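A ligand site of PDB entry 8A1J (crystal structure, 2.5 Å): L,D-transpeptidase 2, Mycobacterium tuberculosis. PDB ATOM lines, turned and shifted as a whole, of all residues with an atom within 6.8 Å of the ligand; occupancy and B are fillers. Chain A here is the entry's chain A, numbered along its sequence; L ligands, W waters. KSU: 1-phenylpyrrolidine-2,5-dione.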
ATOM      1  N   GLY A 228     -35.459  -8.358 -18.980  1.00  0.00           N
ATOM      2  CA  GLY A 228     -35.661  -8.089 -17.577  1.00  0.00           C
ATOM      3  C   GLY A 228     -37.107  -7.753 -17.232  1.00  0.00           C
ATOM      4  O   GLY A 228     -37.737  -6.933 -17.897  1.00  0.00           O
ATOM      5  N   ILE A 249     -20.893 -20.183 -15.952  1.00  0.00           N
ATOM      6  CA  ILE A 249     -21.605 -20.245 -14.683  1.00  0.00           C
ATOM      7  C   ILE A 249     -21.952 -18.813 -14.269  1.00  0.00           C
ATOM      8  O   ILE A 249     -21.067 -17.970 -14.123  1.00  0.00           O
ATOM      9  CB  ILE A 249     -20.780 -20.958 -13.608  1.00  0.00           C
ATOM     10  CG1 ILE A 249     -20.424 -22.365 -14.059  1.00  0.00           C
ATOM     11  CG2 ILE A 249     -21.560 -21.005 -12.297  1.00  0.00           C
ATOM     12  CD1 ILE A 249     -19.659 -23.182 -13.023  1.00  0.00           C
ATOM     13  N   MET A 250     -23.244 -18.551 -14.101  1.00  0.00           N
ATOM     14  CA  MET A 250     -23.724 -17.225 -13.718  1.00  0.00           C
ATOM     15  C   MET A 250     -23.831 -17.174 -12.195  1.00  0.00           C
ATOM     16  O   MET A 250     -24.856 -17.534 -11.618  1.00  0.00           O
ATOM     17  CB  MET A 250     -25.064 -16.925 -14.366  1.00  0.00           C
ATOM     18  CG  MET A 250     -25.058 -16.970 -15.878  1.00  0.00           C
ATOM     19  SD  MET A 250     -23.990 -15.711 -16.596  1.00  0.00           S
ATOM     20  CE  MET A 250     -25.024 -15.121 -17.934  1.00  0.00           C
ATOM     21  N   ASP A 251     -22.758 -16.752 -11.548  1.00  0.00           N
ATOM     22  CA  ASP A 251     -22.751 -16.521 -10.106  1.00  0.00           C
ATOM     23  C   ASP A 251     -23.190 -15.085  -9.863  1.00  0.00           C
ATOM     24  O   ASP A 251     -22.581 -14.136 -10.371  1.00  0.00           O
ATOM     25  CB  ASP A 251     -21.371 -16.777  -9.516  1.00  0.00           C
ATOM     26  CG  ASP A 251     -21.345 -16.599  -8.001  1.00  0.00           C
ATOM     27  OD1 ASP A 251     -22.381 -16.211  -7.421  1.00  0.00           O
ATOM     28  OD2 ASP A 251     -20.289 -16.855  -7.391  1.00  0.00           O
ATOM     29  N   SER A 252     -24.269 -14.920  -9.087  1.00  0.00           N
ATOM     30  CA  SER A 252     -24.776 -13.576  -8.802  1.00  0.00           C
ATOM     31  C   SER A 252     -23.779 -12.762  -7.995  1.00  0.00           C
ATOM     32  O   SER A 252     -23.772 -11.530  -8.075  1.00  0.00           O
ATOM     33  CB  SER A 252     -26.107 -13.669  -8.052  1.00  0.00           C
ATOM     34  OG  SER A 252     -26.527 -12.396  -7.611  1.00  0.00           O
ATOM     35  N   TYR A 255     -21.391  -9.815  -9.326  1.00  0.00           N
ATOM     36  CA  TYR A 255     -21.852  -8.439  -9.451  1.00  0.00           C
ATOM     37  C   TYR A 255     -22.270  -7.855  -8.107  1.00  0.00           C
ATOM     38  O   TYR A 255     -23.032  -6.882  -8.061  1.00  0.00           O
ATOM     39  CB  TYR A 255     -23.012  -8.363 -10.447  1.00  0.00           C
ATOM     40  CG  TYR A 255     -22.731  -9.149 -11.712  1.00  0.00           C
ATOM     41  CD1 TYR A 255     -22.205  -8.527 -12.837  1.00  0.00           C
ATOM     42  CD2 TYR A 255     -22.989 -10.515 -11.764  1.00  0.00           C
ATOM     43  CE1 TYR A 255     -21.948  -9.248 -13.983  1.00  0.00           C
ATOM     44  CE2 TYR A 255     -22.728 -11.240 -12.918  1.00  0.00           C
ATOM     45  CZ  TYR A 255     -22.216 -10.604 -14.021  1.00  0.00           C
ATOM     46  OH  TYR A 255     -21.959 -11.325 -15.167  1.00  0.00           O
ATOM     47  N   ASN A 263     -33.207 -11.658  -5.546  1.00  0.00           N
ATOM     48  CA  ASN A 263     -32.748 -11.350  -6.894  1.00  0.00           C
ATOM     49  C   ASN A 263     -31.408 -11.979  -7.215  1.00  0.00           C
ATOM     50  O   ASN A 263     -30.813 -11.662  -8.249  1.00  0.00           O
ATOM     51  CB  ASN A 263     -32.666  -9.834  -7.079  1.00  0.00           C
ATOM     52  CG  ASN A 263     -34.029  -9.186  -7.110  1.00  0.00           C
ATOM     53  OD1 ASN A 263     -35.039  -9.834  -7.394  1.00  0.00           O
ATOM     54  ND2 ASN A 263     -34.076  -7.887  -6.820  1.00  0.00           N
ATOM     55  N   GLY A 264     -30.920 -12.882  -6.359  1.00  0.00           N
ATOM     56  CA  GLY A 264     -29.686 -13.586  -6.620  1.00  0.00           C
ATOM     57  C   GLY A 264     -29.891 -14.850  -7.435  1.00  0.00           C
ATOM     58  O   GLY A 264     -31.016 -15.251  -7.750  1.00  0.00           O
ATOM     59  N   TYR A 265     -28.783 -15.498  -7.774  1.00  0.00           N
ATOM     60  CA  TYR A 265     -28.823 -16.671  -8.634  1.00  0.00           C
ATOM     61  C   TYR A 265     -27.452 -17.297  -8.788  1.00  0.00           C
ATOM     62  O   TYR A 265     -26.440 -16.585  -8.828  1.00  0.00           O
ATOM     63  CB  TYR A 265     -29.370 -16.277 -10.015  1.00  0.00           C
ATOM     64  CG  TYR A 265     -28.693 -15.060 -10.611  1.00  0.00           C
ATOM     65  CD1 TYR A 265     -27.489 -15.161 -11.291  1.00  0.00           C
ATOM     66  CD2 TYR A 265     -29.263 -13.796 -10.478  1.00  0.00           C
ATOM     67  CE1 TYR A 265     -26.879 -14.061 -11.842  1.00  0.00           C
ATOM     68  CE2 TYR A 265     -28.652 -12.679 -11.025  1.00  0.00           C
ATOM     69  CZ  TYR A 265     -27.465 -12.814 -11.708  1.00  0.00           C
ATOM     70  OH  TYR A 265     -26.851 -11.704 -12.249  1.00  0.00           O
ATOM     71  N   ARG A 266     -27.406 -18.630  -8.894  1.00  0.00           N
ATOM     72  CA  ARG A 266     -26.154 -19.319  -9.208  1.00  0.00           C
ATOM     73  C   ARG A 266     -26.514 -20.549 -10.037  1.00  0.00           C
ATOM     74  O   ARG A 266     -26.766 -21.629  -9.496  1.00  0.00           O
ATOM     75  CB  ARG A 266     -25.387 -19.705  -7.945  1.00  0.00           C
ATOM     76  CG  ARG A 266     -24.178 -20.579  -8.208  1.00  0.00           C
ATOM     77  CD  ARG A 266     -23.381 -20.793  -6.928  1.00  0.00           C
ATOM     78  NE  ARG A 266     -24.243 -21.182  -5.819  1.00  0.00           N
ATOM     79  CZ  ARG A 266     -24.001 -20.906  -4.536  1.00  0.00           C
ATOM     80  NH1 ARG A 266     -22.913 -20.234  -4.203  1.00  0.00           N
ATOM     81  NH2 ARG A 266     -24.854 -21.297  -3.610  1.00  0.00           N
ATOM     82  N   THR A 267     -26.542 -20.361 -11.354  1.00  0.00           N
ATOM     83  CA  THR A 267     -26.852 -21.438 -12.276  1.00  0.00           C
ATOM     84  C   THR A 267     -25.883 -21.385 -13.439  1.00  0.00           C
ATOM     85  O   THR A 267     -25.190 -20.382 -13.656  1.00  0.00           O
ATOM     86  CB  THR A 267     -28.298 -21.369 -12.777  1.00  0.00           C
ATOM     87  OG1 THR A 267     -28.511 -22.365 -13.781  1.00  0.00           O
ATOM     88  CG2 THR A 267     -28.605 -20.000 -13.365  1.00  0.00           C
ATOM     89  N   VAL A 269     -25.506 -21.604 -17.484  1.00  0.00           N
ATOM     90  CA  VAL A 269     -26.231 -21.408 -18.733  1.00  0.00           C
ATOM     91  C   VAL A 269     -25.269 -21.646 -19.890  1.00  0.00           C
ATOM     92  O   VAL A 269     -24.046 -21.658 -19.735  1.00  0.00           O
ATOM     93  CB  VAL A 269     -26.872 -20.016 -18.837  1.00  0.00           C
ATOM     94  CG1 VAL A 269     -27.711 -19.731 -17.588  1.00  0.00           C
ATOM     95  CG2 VAL A 269     -25.809 -18.948 -19.030  1.00  0.00           C
ATOM     96  N   SER A 278     -22.186  -4.869 -16.116  1.00  0.00           N
ATOM     97  CA  SER A 278     -23.151  -4.931 -15.026  1.00  0.00           C
ATOM     98  C   SER A 278     -23.970  -6.207 -15.028  1.00  0.00           C
ATOM     99  O   SER A 278     -24.781  -6.392 -14.110  1.00  0.00           O
ATOM    100  CB  SER A 278     -24.085  -3.720 -15.083  1.00  0.00           C
ATOM    101  OG  SER A 278     -25.018  -3.851 -16.137  1.00  0.00           O
ATOM    102  N   GLY A 279     -23.808  -7.079 -16.016  1.00  0.00           N
ATOM    103  CA  GLY A 279     -24.409  -8.396 -15.999  1.00  0.00           C
ATOM    104  C   GLY A 279     -25.337  -8.719 -17.156  1.00  0.00           C
ATOM    105  O   GLY A 279     -25.760  -9.879 -17.272  1.00  0.00           O
ATOM    106  N   VAL A 280     -25.680  -7.771 -18.028  1.00  0.00           N
ATOM    107  CA  VAL A 280     -26.588  -8.072 -19.133  1.00  0.00           C
ATOM    108  C   VAL A 280     -25.894  -9.014 -20.109  1.00  0.00           C
ATOM    109  O   VAL A 280     -24.720  -8.810 -20.462  1.00  0.00           O
ATOM    110  CB  VAL A 280     -27.049  -6.776 -19.817  1.00  0.00           C
ATOM    111  CG1 VAL A 280     -28.140  -7.076 -20.824  1.00  0.00           C
ATOM    112  CG2 VAL A 280     -27.525  -5.770 -18.779  1.00  0.00           C
ATOM    113  N   PHE A 281     -26.610 -10.053 -20.534  1.00  0.00           N
ATOM    114  CA  PHE A 281     -26.070 -11.069 -21.415  1.00  0.00           C
ATOM    115  C   PHE A 281     -27.074 -11.392 -22.513  1.00  0.00           C
ATOM    116  O   PHE A 281     -28.230 -10.967 -22.469  1.00  0.00           O
ATOM    117  CB  PHE A 281     -25.757 -12.367 -20.664  1.00  0.00           C
ATOM    118  CG  PHE A 281     -24.357 -12.459 -20.125  1.00  0.00           C
ATOM    119  CD1 PHE A 281     -24.022 -11.860 -18.921  1.00  0.00           C
ATOM    120  CD2 PHE A 281     -23.407 -13.200 -20.792  1.00  0.00           C
ATOM    121  CE1 PHE A 281     -22.742 -11.968 -18.422  1.00  0.00           C
ATOM    122  CE2 PHE A 281     -22.123 -13.313 -20.301  1.00  0.00           C
ATOM    123  CZ  PHE A 281     -21.800 -12.704 -19.112  1.00  0.00           C
ATOM    124  N   HIS A 283     -28.010 -15.135 -23.694  1.00  0.00           N
ATOM    125  CA  HIS A 283     -27.705 -16.515 -23.357  1.00  0.00           C
ATOM    126  C   HIS A 283     -28.865 -17.427 -23.760  1.00  0.00           C
ATOM    127  O   HIS A 283     -29.938 -16.979 -24.151  1.00  0.00           O
ATOM    128  CB  HIS A 283     -27.417 -16.675 -21.860  1.00  0.00           C
ATOM    129  CG  HIS A 283     -28.617 -16.450 -20.985  1.00  0.00           C
ATOM    130  ND1 HIS A 283     -29.345 -17.478 -20.450  1.00  0.00           N
ATOM    131  CD2 HIS A 283     -29.201 -15.303 -20.556  1.00  0.00           C
ATOM    132  CE1 HIS A 283     -30.340 -16.991 -19.718  1.00  0.00           C
ATOM    133  NE2 HIS A 283     -30.273 -15.668 -19.776  1.00  0.00           N
ATOM    134  N   SER A 284     -28.609 -18.738 -23.661  1.00  0.00           N
ATOM    135  CA  SER A 284     -29.633 -19.737 -23.880  1.00  0.00           C
ATOM    136  C   SER A 284     -30.479 -19.892 -22.625  1.00  0.00           C
ATOM    137  O   SER A 284     -29.954 -20.091 -21.532  1.00  0.00           O
ATOM    138  CB  SER A 284     -28.994 -21.078 -24.257  1.00  0.00           C
ATOM    139  OG  SER A 284     -29.924 -22.136 -24.132  1.00  0.00           O
ATOM    140  N   ALA A 285     -31.801 -19.806 -22.784  1.00  0.00           N
ATOM    141  CA  ALA A 285     -32.747 -19.890 -21.681  1.00  0.00           C
ATOM    142  C   ALA A 285     -33.886 -20.824 -22.070  1.00  0.00           C
ATOM    143  O   ALA A 285     -34.949 -20.376 -22.496  1.00  0.00           O
ATOM    144  CB  ALA A 285     -33.278 -18.512 -21.298  1.00  0.00           C
ATOM    145  N   TRP A 287     -35.906 -22.471 -20.179  1.00  0.00           N
ATOM    146  CA  TRP A 287     -37.028 -22.344 -19.272  1.00  0.00           C
ATOM    147  C   TRP A 287     -37.940 -21.163 -19.580  1.00  0.00           C
ATOM    148  O   TRP A 287     -38.867 -20.911 -18.802  1.00  0.00           O
ATOM    149  CB  TRP A 287     -36.514 -22.211 -17.842  1.00  0.00           C
ATOM    150  CG  TRP A 287     -35.654 -20.986 -17.646  1.00  0.00           C
ATOM    151  CD1 TRP A 287     -36.076 -19.737 -17.312  1.00  0.00           C
ATOM    152  CD2 TRP A 287     -34.230 -20.903 -17.786  1.00  0.00           C
ATOM    153  NE1 TRP A 287     -35.006 -18.871 -17.236  1.00  0.00           N
ATOM    154  CE2 TRP A 287     -33.859 -19.573 -17.528  1.00  0.00           C
ATOM    155  CE3 TRP A 287     -33.232 -21.828 -18.114  1.00  0.00           C
ATOM    156  CZ2 TRP A 287     -32.534 -19.147 -17.574  1.00  0.00           C
ATOM    157  CZ3 TRP A 287     -31.918 -21.399 -18.168  1.00  0.00           C
ATOM    158  CH2 TRP A 287     -31.587 -20.069 -17.896  1.00  0.00           C
ATOM    159  N   SER A 298     -36.868 -12.213 -16.685  1.00  0.00           N
ATOM    160  CA  SER A 298     -35.450 -12.410 -16.406  1.00  0.00           C
ATOM    161  C   SER A 298     -34.948 -11.331 -15.455  1.00  0.00           C
ATOM    162  O   SER A 298     -35.672 -10.406 -15.097  1.00  0.00           O
ATOM    163  CB  SER A 298     -34.617 -12.408 -17.693  1.00  0.00           C
ATOM    164  OG  SER A 298     -34.456 -11.096 -18.198  1.00  0.00           O
ATOM    165  N   HIS A 299     -33.681 -11.461 -15.074  1.00  0.00           N
ATOM    166  CA  HIS A 299     -33.008 -10.510 -14.146  1.00  0.00           C
ATOM    167  C   HIS A 299     -32.321  -9.385 -14.919  1.00  0.00           C
ATOM    168  O   HIS A 299     -31.774  -8.481 -14.274  1.00  0.00           O
ATOM    169  CB  HIS A 299     -31.968 -11.248 -13.306  1.00  0.00           C
ATOM    170  CG  HIS A 299     -32.553 -12.202 -12.318  1.00  0.00           C
ATOM    171  ND1 HIS A 299     -32.876 -13.489 -12.653  1.00  0.00           N
ATOM    172  CD2 HIS A 299     -32.843 -12.065 -11.010  1.00  0.00           C
ATOM    173  CE1 HIS A 299     -33.363 -14.097 -11.606  1.00  0.00           C
ATOM    174  NE2 HIS A 299     -33.342 -13.253 -10.588  1.00  0.00           N
ATOM    175  N   GLY A 300     -32.364  -9.417 -16.254  1.00  0.00           N
ATOM    176  CA  GLY A 300     -31.697  -8.377 -17.041  1.00  0.00           C
ATOM    177  C   GLY A 300     -31.132  -8.880 -18.356  1.00  0.00           C
ATOM    178  O   GLY A 300     -31.285  -8.172 -19.343  1.00  0.00           O
ATOM    179  N   CYS A 301     -30.575 -10.102 -18.402  1.00  0.00           N
ATOM    180  CA  CYS A 301     -30.020 -10.605 -19.683  1.00  0.00           C
ATOM    181  C   CYS A 301     -31.138 -10.991 -20.639  1.00  0.00           C
ATOM    182  O   CYS A 301     -32.265 -11.242 -20.198  1.00  0.00           O
ATOM    183  CB  CYS A 301     -29.044 -11.765 -19.549  1.00  0.00           C
ATOM    184  SG  CYS A 301     -28.032 -11.640 -18.034  1.00  0.00           S
ATOM    185  N   LEU A 302     -30.819 -11.015 -21.934  1.00  0.00           N
ATOM    186  CA  LEU A 302     -31.848 -11.345 -22.935  1.00  0.00           C
ATOM    187  C   LEU A 302     -31.948 -12.860 -23.047  1.00  0.00           C
ATOM    188  O   LEU A 302     -30.995 -13.487 -23.500  1.00  0.00           O
ATOM    189  CB  LEU A 302     -31.447 -10.688 -24.260  1.00  0.00           C
ATOM    190  CG  LEU A 302     -31.640  -9.172 -24.314  1.00  0.00           C
ATOM    191  CD1 LEU A 302     -31.568  -8.527 -22.945  1.00  0.00           C
ATOM    192  CD2 LEU A 302     -30.638  -8.514 -25.246  1.00  0.00           C
ATOM    193  N   ASN A 303     -33.088 -13.404 -22.616  1.00  0.00           N
ATOM    194  CA  ASN A 303     -33.391 -14.861 -22.666  1.00  0.00           C
ATOM    195  C   ASN A 303     -33.668 -15.214 -24.125  1.00  0.00           C
ATOM    196  O   ASN A 303     -34.480 -14.536 -24.750  1.00  0.00           O
ATOM    197  CB  ASN A 303     -34.568 -15.222 -21.780  1.00  0.00           C
ATOM    198  CG  ASN A 303     -34.200 -15.358 -20.315  1.00  0.00           C
ATOM    199  OD1 ASN A 303     -33.215 -14.796 -19.869  1.00  0.00           O
ATOM    200  ND2 ASN A 303     -34.999 -16.094 -19.565  1.00  0.00           N
HETATM  201  C10 KSU L   1     -30.913 -16.410 -13.363  1.00  0.00           C
HETATM  202  C13 KSU L   1     -29.619 -16.237 -15.909  1.00  0.00           C
HETATM  203  C15 KSU L   1     -27.374 -11.933 -15.438  1.00  0.00           C
HETATM  204  C05 KSU L   1     -28.557 -11.582 -16.273  1.00  0.00           C
HETATM  205  C06 KSU L   1     -29.634 -12.618 -16.054  1.00  0.00           C
HETATM  206  C08 KSU L   1     -29.631 -15.037 -14.964  1.00  0.00           C
HETATM  207  C09 KSU L   1     -30.231 -15.108 -13.779  1.00  0.00           C
HETATM  208  C11 KSU L   1     -30.905 -17.461 -14.175  1.00  0.00           C
HETATM  209  C12 KSU L   1     -30.214 -17.369 -15.545  1.00  0.00           C
HETATM  210  C14 KSU L   1     -27.508 -13.445 -15.167  1.00  0.00           C
HETATM  211  N07 KSU L   1     -28.982 -13.788 -15.368  1.00  0.00           N
HETATM  212  O16 KSU L   1     -26.642 -14.193 -14.868  1.00  0.00           O
HETATM  213  O17 KSU L   1     -30.773 -12.518 -16.374  1.00  0.00           O
HETATM  214  O   HOH W   1     -32.924 -14.784 -15.432  1.00  0.00           O
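N of Cys 301 lies within hydrogen-bond range of O17 of the ligand (3.2 Å). The backbone NH (N) of Gly 300 sits at hydrogen-bond distance from an oxygen (O17) of the ligand. The side-chain sulfur (SG) of Cys 301 is covalently linked to a carbon (C05) of the ligand, 1.8 Å away. N of His 299 sits at hydrogen-bond distance from O17 of the ligand (3.4 Å).
The side-chain hydroxyl (OG) of Ser 298 is in hydrogen-bond range of the backbone NH (N) of Gly 300. The side-chain sulfur (SG) of Cys 301 lies close to the backbone NH (N) of Phe 281, 3.3 Å away. N of Met 250 is in hydrogen-bond range of O of Thr 267, 2.7 Å away. N of His 283 lies within hydrogen-bond range of O of Leu 302, at 3.4 Å. A ring nitrogen (NE2) of His 283 sits at hydrogen-bond distance from the side-chain amide oxygen (OD1) of Asn 303 (3.1 Å). N of Ser 252 lies within hydrogen-bond range of O of Tyr 265, 2.7 Å away. OG of Ser 298 sits at hydrogen-bond distance from O of Cys 301.
An oxygen (O16) of the ligand sits close to the side-chain sulfur (SD) of Met 250 (3.5 Å). Residues that only touch the ligand: Tyr 265 (3.0 Å), Gly 279 (3.2 Å), Thr 267 (3.5 Å), Trp 287 (3.6 Å) and His 283 (3.9 Å). Hydrophobic or aromatic side chains within 4 Å of the ligand: Met 250, Tyr 265, His 283, Trp 287 and His 299. The nearest printed residue that does not touch the ligand is Val 269 (4.002 Å).
Water W1 bridges ND1 of His 299 (3.1 Å) and O17 of the ligand (3.3 Å).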
